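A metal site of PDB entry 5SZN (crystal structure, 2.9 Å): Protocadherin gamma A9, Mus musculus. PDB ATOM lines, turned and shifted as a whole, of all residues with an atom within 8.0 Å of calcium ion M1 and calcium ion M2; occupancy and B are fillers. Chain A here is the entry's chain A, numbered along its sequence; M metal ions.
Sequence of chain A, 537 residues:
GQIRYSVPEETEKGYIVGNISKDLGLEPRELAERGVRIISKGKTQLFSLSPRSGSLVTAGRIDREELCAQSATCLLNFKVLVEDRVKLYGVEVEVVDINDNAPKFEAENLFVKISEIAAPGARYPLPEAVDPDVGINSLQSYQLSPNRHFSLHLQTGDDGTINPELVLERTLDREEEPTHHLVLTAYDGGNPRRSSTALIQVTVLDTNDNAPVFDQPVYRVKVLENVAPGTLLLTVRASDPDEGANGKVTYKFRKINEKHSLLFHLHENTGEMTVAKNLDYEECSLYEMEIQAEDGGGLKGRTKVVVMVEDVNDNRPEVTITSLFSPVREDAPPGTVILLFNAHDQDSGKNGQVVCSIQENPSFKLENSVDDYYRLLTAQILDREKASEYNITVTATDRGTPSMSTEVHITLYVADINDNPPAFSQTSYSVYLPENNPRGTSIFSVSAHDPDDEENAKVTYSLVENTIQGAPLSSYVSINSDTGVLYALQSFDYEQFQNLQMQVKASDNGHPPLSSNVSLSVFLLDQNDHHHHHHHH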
ATOM      1  N   GLU A   9     -31.073  13.915   3.579  1.00  0.00           N
ATOM      2  CA  GLU A   9     -29.844  14.262   4.258  1.00  0.00           C
ATOM      3  C   GLU A   9     -29.908  15.678   4.817  1.00  0.00           C
ATOM      4  O   GLU A   9     -30.688  16.525   4.352  1.00  0.00           O
ATOM      5  CB  GLU A   9     -28.649  14.157   3.308  1.00  0.00           C
ATOM      6  CG  GLU A   9     -28.786  15.022   2.073  1.00  0.00           C
ATOM      7  CD  GLU A   9     -27.461  15.227   1.359  1.00  0.00           C
ATOM      8  OE1 GLU A   9     -26.411  15.230   2.027  1.00  0.00           O
ATOM      9  OE2 GLU A   9     -27.488  15.370   0.118  1.00  0.00           O
ATOM     10  N   GLU A  10     -29.070  15.930   5.815  1.00  0.00           N
ATOM     11  CA  GLU A  10     -28.940  17.241   6.446  1.00  0.00           C
ATOM     12  C   GLU A  10     -30.285  17.797   6.890  1.00  0.00           C
ATOM     13  O   GLU A  10     -30.645  18.946   6.636  1.00  0.00           O
ATOM     14  CB  GLU A  10     -28.215  18.217   5.518  1.00  0.00           C
ATOM     15  CG  GLU A  10     -26.766  17.853   5.271  1.00  0.00           C
ATOM     16  CD  GLU A  10     -26.036  18.916   4.479  1.00  0.00           C
ATOM     17  OE1 GLU A  10     -26.704  19.802   3.916  1.00  0.00           O
ATOM     18  OE2 GLU A  10     -24.788  18.856   4.415  1.00  0.00           O
ATOM     19  N   ILE A  62     -27.213  14.555   9.194  1.00  0.00           N
ATOM     20  CA  ILE A  62     -26.680  13.529   8.296  1.00  0.00           C
ATOM     21  C   ILE A  62     -26.177  14.202   7.034  1.00  0.00           C
ATOM     22  O   ILE A  62     -26.941  14.851   6.314  1.00  0.00           O
ATOM     23  CB  ILE A  62     -27.745  12.474   7.938  1.00  0.00           C
ATOM     24  CG1 ILE A  62     -28.231  11.743   9.184  1.00  0.00           C
ATOM     25  CG2 ILE A  62     -27.191  11.485   6.922  1.00  0.00           C
ATOM     26  CD1 ILE A  62     -29.549  12.246   9.704  1.00  0.00           C
ATOM     27  N   ASP A  63     -24.888  14.033   6.753  1.00  0.00           N
ATOM     28  CA  ASP A  63     -24.286  14.496   5.504  1.00  0.00           C
ATOM     29  C   ASP A  63     -23.672  13.273   4.825  1.00  0.00           C
ATOM     30  O   ASP A  63     -22.569  12.852   5.160  1.00  0.00           O
ATOM     31  CB  ASP A  63     -23.242  15.577   5.743  1.00  0.00           C
ATOM     32  CG  ASP A  63     -22.503  15.983   4.483  1.00  0.00           C
ATOM     33  OD1 ASP A  63     -23.059  16.784   3.703  1.00  0.00           O
ATOM     34  OD2 ASP A  63     -21.381  15.487   4.270  1.00  0.00           O
ATOM     35  N   ARG A  64     -24.406  12.702   3.857  1.00  0.00           N
ATOM     36  CA  ARG A  64     -23.951  11.495   3.188  1.00  0.00           C
ATOM     37  C   ARG A  64     -22.656  11.718   2.404  1.00  0.00           C
ATOM     38  O   ARG A  64     -21.973  10.742   2.066  1.00  0.00           O
ATOM     39  CB  ARG A  64     -25.034  10.957   2.254  1.00  0.00           C
ATOM     40  CG  ARG A  64     -25.658  12.008   1.356  1.00  0.00           C
ATOM     41  CD  ARG A  64     -26.339  11.364   0.166  1.00  0.00           C
ATOM     42  NE  ARG A  64     -25.414  10.515  -0.567  1.00  0.00           N
ATOM     43  CZ  ARG A  64     -24.539  10.950  -1.466  1.00  0.00           C
ATOM     44  NH1 ARG A  64     -24.460  12.252  -1.740  1.00  0.00           N
ATOM     45  NH2 ARG A  64     -23.732  10.104  -2.084  1.00  0.00           N
ATOM     46  N   GLU A  65     -22.309  12.977   2.112  1.00  0.00           N
ATOM     47  CA  GLU A  65     -21.008  13.257   1.521  1.00  0.00           C
ATOM     48  C   GLU A  65     -19.884  12.920   2.488  1.00  0.00           C
ATOM     49  O   GLU A  65     -18.799  12.519   2.067  1.00  0.00           O
ATOM     50  CB  GLU A  65     -20.932  14.721   1.083  1.00  0.00           C
ATOM     51  CG  GLU A  65     -21.768  15.078  -0.127  1.00  0.00           C
ATOM     52  CD  GLU A  65     -23.260  15.032   0.148  1.00  0.00           C
ATOM     53  OE1 GLU A  65     -23.652  15.106   1.336  1.00  0.00           O
ATOM     54  OE2 GLU A  65     -24.049  14.925  -0.810  1.00  0.00           O
ATOM     55  N   GLU A  66     -20.118  13.094   3.792  1.00  0.00           N
ATOM     56  CA  GLU A  66     -19.198  12.667   4.829  1.00  0.00           C
ATOM     57  C   GLU A  66     -19.443  11.234   5.277  1.00  0.00           C
ATOM     58  O   GLU A  66     -18.863  10.806   6.282  1.00  0.00           O
ATOM     59  CB  GLU A  66     -19.271  13.615   6.030  1.00  0.00           C
ATOM     60  N   ALA A  69     -19.755   9.552   0.488  1.00  0.00           N
ATOM     61  CA  ALA A  69     -19.022  10.345  -0.490  1.00  0.00           C
ATOM     62  C   ALA A  69     -19.691  10.323  -1.863  1.00  0.00           C
ATOM     63  O   ALA A  69     -20.676  11.031  -2.091  1.00  0.00           O
ATOM     64  CB  ALA A  69     -17.577   9.870  -0.592  1.00  0.00           C
ATOM     65  N   VAL A  96     -31.181   9.824   1.131  1.00  0.00           N
ATOM     66  CA  VAL A  96     -31.277  10.372  -0.222  1.00  0.00           C
ATOM     67  C   VAL A  96     -30.331  11.548  -0.325  1.00  0.00           C
ATOM     68  O   VAL A  96     -29.811  12.030   0.684  1.00  0.00           O
ATOM     69  CB  VAL A  96     -32.721  10.777  -0.575  1.00  0.00           C
ATOM     70  CG1 VAL A  96     -33.697   9.697  -0.135  1.00  0.00           C
ATOM     71  CG2 VAL A  96     -33.060  12.114   0.048  1.00  0.00           C
ATOM     72  N   ASP A  97     -30.089  12.030  -1.542  1.00  0.00           N
ATOM     73  CA  ASP A  97     -29.179  13.135  -1.782  1.00  0.00           C
ATOM     74  C   ASP A  97     -29.955  14.388  -2.147  1.00  0.00           C
ATOM     75  O   ASP A  97     -30.899  14.341  -2.946  1.00  0.00           O
ATOM     76  CB  ASP A  97     -28.179  12.797  -2.886  1.00  0.00           C
ATOM     77  CG  ASP A  97     -27.140  13.887  -3.092  1.00  0.00           C
ATOM     78  OD1 ASP A  97     -26.092  13.840  -2.404  1.00  0.00           O
ATOM     79  OD2 ASP A  97     -27.360  14.785  -3.929  1.00  0.00           O
ATOM     80  N   ILE A  98     -29.554  15.508  -1.547  1.00  0.00           N
ATOM     81  CA  ILE A  98     -30.066  16.824  -1.906  1.00  0.00           C
ATOM     82  C   ILE A  98     -28.893  17.668  -2.398  1.00  0.00           C
ATOM     83  O   ILE A  98     -27.733  17.400  -2.073  1.00  0.00           O
ATOM     84  CB  ILE A  98     -30.795  17.520  -0.742  1.00  0.00           C
ATOM     85  CG1 ILE A  98     -29.796  17.951   0.338  1.00  0.00           C
ATOM     86  CG2 ILE A  98     -31.861  16.596  -0.155  1.00  0.00           C
ATOM     87  CD1 ILE A  98     -30.439  18.540   1.568  1.00  0.00           C
ATOM     88  N   ASN A  99     -29.217  18.684  -3.187  1.00  0.00           N
ATOM     89  CA  ASN A  99     -28.195  19.540  -3.791  1.00  0.00           C
ATOM     90  C   ASN A  99     -27.899  20.696  -2.848  1.00  0.00           C
ATOM     91  O   ASN A  99     -28.583  21.727  -2.862  1.00  0.00           O
ATOM     92  CB  ASN A  99     -28.625  20.029  -5.163  1.00  0.00           C
ATOM     93  CG  ASN A  99     -27.547  20.843  -5.854  1.00  0.00           C
ATOM     94  OD1 ASN A  99     -26.357  20.579  -5.684  1.00  0.00           O
ATOM     95  ND2 ASN A  99     -27.961  21.842  -6.621  1.00  0.00           N
ATOM     96  N   ASP A 100     -26.876  20.539  -2.015  1.00  0.00           N
ATOM     97  CA  ASP A 100     -26.395  21.603  -1.162  1.00  0.00           C
ATOM     98  C   ASP A 100     -24.963  22.021  -1.452  1.00  0.00           C
ATOM     99  O   ASP A 100     -24.576  23.135  -1.092  1.00  0.00           O
ATOM    100  CB  ASP A 100     -26.490  21.189   0.325  1.00  0.00           C
ATOM    101  CG  ASP A 100     -25.747  19.904   0.612  1.00  0.00           C
ATOM    102  OD1 ASP A 100     -25.799  18.986  -0.226  1.00  0.00           O
ATOM    103  OD2 ASP A 100     -25.089  19.810   1.670  1.00  0.00           O
ATOM    104  N   ASN A 101     -24.168  21.162  -2.085  1.00  0.00           N
ATOM    105  CA  ASN A 101     -22.763  21.440  -2.365  1.00  0.00           C
ATOM    106  C   ASN A 101     -22.620  21.990  -3.777  1.00  0.00           C
ATOM    107  O   ASN A 101     -23.249  21.505  -4.721  1.00  0.00           O
ATOM    108  CB  ASN A 101     -21.921  20.169  -2.220  1.00  0.00           C
ATOM    109  CG  ASN A 101     -21.684  19.794  -0.764  1.00  0.00           C
ATOM    110  OD1 ASN A 101     -20.684  19.152  -0.435  1.00  0.00           O
ATOM    111  ND2 ASN A 101     -22.592  20.197   0.109  1.00  0.00           N
ATOM    112  N   ASP A 131     -17.947  17.757  -7.864  1.00  0.00           N
ATOM    113  CA  ASP A 131     -19.133  18.059  -7.084  1.00  0.00           C
ATOM    114  C   ASP A 131     -19.377  16.893  -6.131  1.00  0.00           C
ATOM    115  O   ASP A 131     -19.547  15.742  -6.594  1.00  0.00           O
ATOM    116  CB  ASP A 131     -20.343  18.293  -7.990  1.00  0.00           C
ATOM    117  CG  ASP A 131     -21.570  18.754  -7.219  1.00  0.00           C
ATOM    118  OD1 ASP A 131     -21.432  19.174  -6.059  1.00  0.00           O
ATOM    119  OD2 ASP A 131     -22.681  18.715  -7.796  1.00  0.00           O
ATOM    120  N   PRO A 132     -19.388  17.125  -4.814  1.00  0.00           N
ATOM    121  CA  PRO A 132     -19.579  16.005  -3.868  1.00  0.00           C
ATOM    122  C   PRO A 132     -20.894  15.262  -4.036  1.00  0.00           C
ATOM    123  O   PRO A 132     -20.974  14.098  -3.644  1.00  0.00           O
ATOM    124  CB  PRO A 132     -19.494  16.690  -2.500  1.00  0.00           C
ATOM    125  CG  PRO A 132     -18.697  17.922  -2.742  1.00  0.00           C
ATOM    126  CD  PRO A 132     -19.059  18.386  -4.123  1.00  0.00           C
ATOM    127  N   ASP A 133     -21.918  15.892  -4.612  1.00  0.00           N
ATOM    128  CA  ASP A 133     -23.217  15.261  -4.748  1.00  0.00           C
ATOM    129  C   ASP A 133     -23.162  14.146  -5.792  1.00  0.00           C
ATOM    130  O   ASP A 133     -22.151  13.913  -6.461  1.00  0.00           O
ATOM    131  CB  ASP A 133     -24.275  16.303  -5.104  1.00  0.00           C
ATOM    132  CG  ASP A 133     -24.371  17.407  -4.074  1.00  0.00           C
ATOM    133  OD1 ASP A 133     -24.192  17.123  -2.876  1.00  0.00           O
ATOM    134  OD2 ASP A 133     -24.611  18.575  -4.463  1.00  0.00           O
ATOM    135  N   VAL A 134     -24.285  13.427  -5.926  1.00  0.00           N
ATOM    136  CA  VAL A 134     -24.390  12.280  -6.820  1.00  0.00           C
ATOM    137  C   VAL A 134     -25.675  12.401  -7.631  1.00  0.00           C
ATOM    138  O   VAL A 134     -26.706  12.831  -7.103  1.00  0.00           O
ATOM    139  CB  VAL A 134     -24.364  10.948  -6.032  1.00  0.00           C
ATOM    140  CG1 VAL A 134     -24.582   9.765  -6.955  1.00  0.00           C
ATOM    141  CG2 VAL A 134     -23.061  10.798  -5.265  1.00  0.00           C
ATOM    142  N   ASN A 137     -27.931  16.017  -8.763  1.00  0.00           N
ATOM    143  CA  ASN A 137     -27.333  17.039  -7.906  1.00  0.00           C
ATOM    144  C   ASN A 137     -25.835  17.197  -8.149  1.00  0.00           C
ATOM    145  O   ASN A 137     -25.262  18.213  -7.723  1.00  0.00           O
ATOM    146  CB  ASN A 137     -27.585  16.698  -6.436  1.00  0.00           C
ATOM    147  CG  ASN A 137     -29.061  16.550  -6.122  1.00  0.00           C
ATOM    148  OD1 ASN A 137     -29.918  17.145  -6.772  1.00  0.00           O
ATOM    149  ND2 ASN A 137     -29.374  15.747  -5.106  1.00  0.00           N
HETATM  150 CA    CA M   1     -25.703  16.665  -0.697  1.00  0.00          CA
HETATM  151 CA    CA M   2     -24.381  17.386   1.749  1.00  0.00          CA
HETATM  152 CA    CA M   3     -23.904  20.272  -6.760  1.00  0.00          CA
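OD1 of Asp 97 touches calcium ion M1, 3.3 Å away.
Six residues have an atom within 4 Å of calcium ion M1: Glu 9, Glu 65, Asp 97, Ile 98, Asp 100 and Asp 133.
The nearest printed residue that does not touch calcium ion M1 is Arg 64 (4.7 Å).
Calcium ion M2 is bound by OE1 of Glu 65 (2.4 Å), OD1 of Asp 63 (2.4 Å) and OD2 of Asp 100 (2.5 Å).
Slightly farther from calcium ion M2 lies OD1 of Asp 100 (2.9 Å).
Slightly farther from calcium ion M2 lies the side-chain carboxylate (OE1) of Glu 9 (3.0 Å).
Slightly farther from calcium ion M2 lies the side-chain carboxylate (OE2) of Glu 10 (3.1 Å).
Asn 101 touches calcium ion M2.
Within 4 Å of calcium ion M2: Glu 9, Glu 10, Asp 63, Glu 65, Asp 100 and Asn 101.
The nearest printed residue that does not touch calcium ion M2 is Asp 133 (4.6 Å).
The side-chain amide oxygen (OD1) of Asn 99 lies close to the side-chain carboxylate (OD2) of Asp 133.
The guanidinium group (NE) of Arg 64 lies within salt-bridge range of the side-chain carboxylate (OD1) of Asp 97, 3.9 Å away.
The side-chain carboxylate (OD2) of Asp 97 is in hydrogen-bond range of the side-chain amide nitrogen (ND2) of Asn 137.
The backbone NH of Glu 66 is in hydrogen-bond range of the side-chain carboxylate of Asp 63.
O of Ile 62 sits at hydrogen-bond distance from N of Glu 10, 2.4 Å away.
The side-chain carboxylate (OE2) of Glu 65 sits close to the guanidinium group (NH1) of Arg 64.
ND2 of Asn 101 lies close to OD2 of Asp 100, 3.0 Å away.
Calcium ion M1 is bound by the side-chain carboxylate (OE2) of Glu 9, the side-chain carboxylate (OD1) of Asp 100, the side-chain carboxylate (OE2) of Glu 65, the backbone carbonyl oxygen (O) of Ile 98 and the side-chain carboxylate (OD1) of Asp 133.
Calcium ion M1 has five donor atoms within binding distance.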
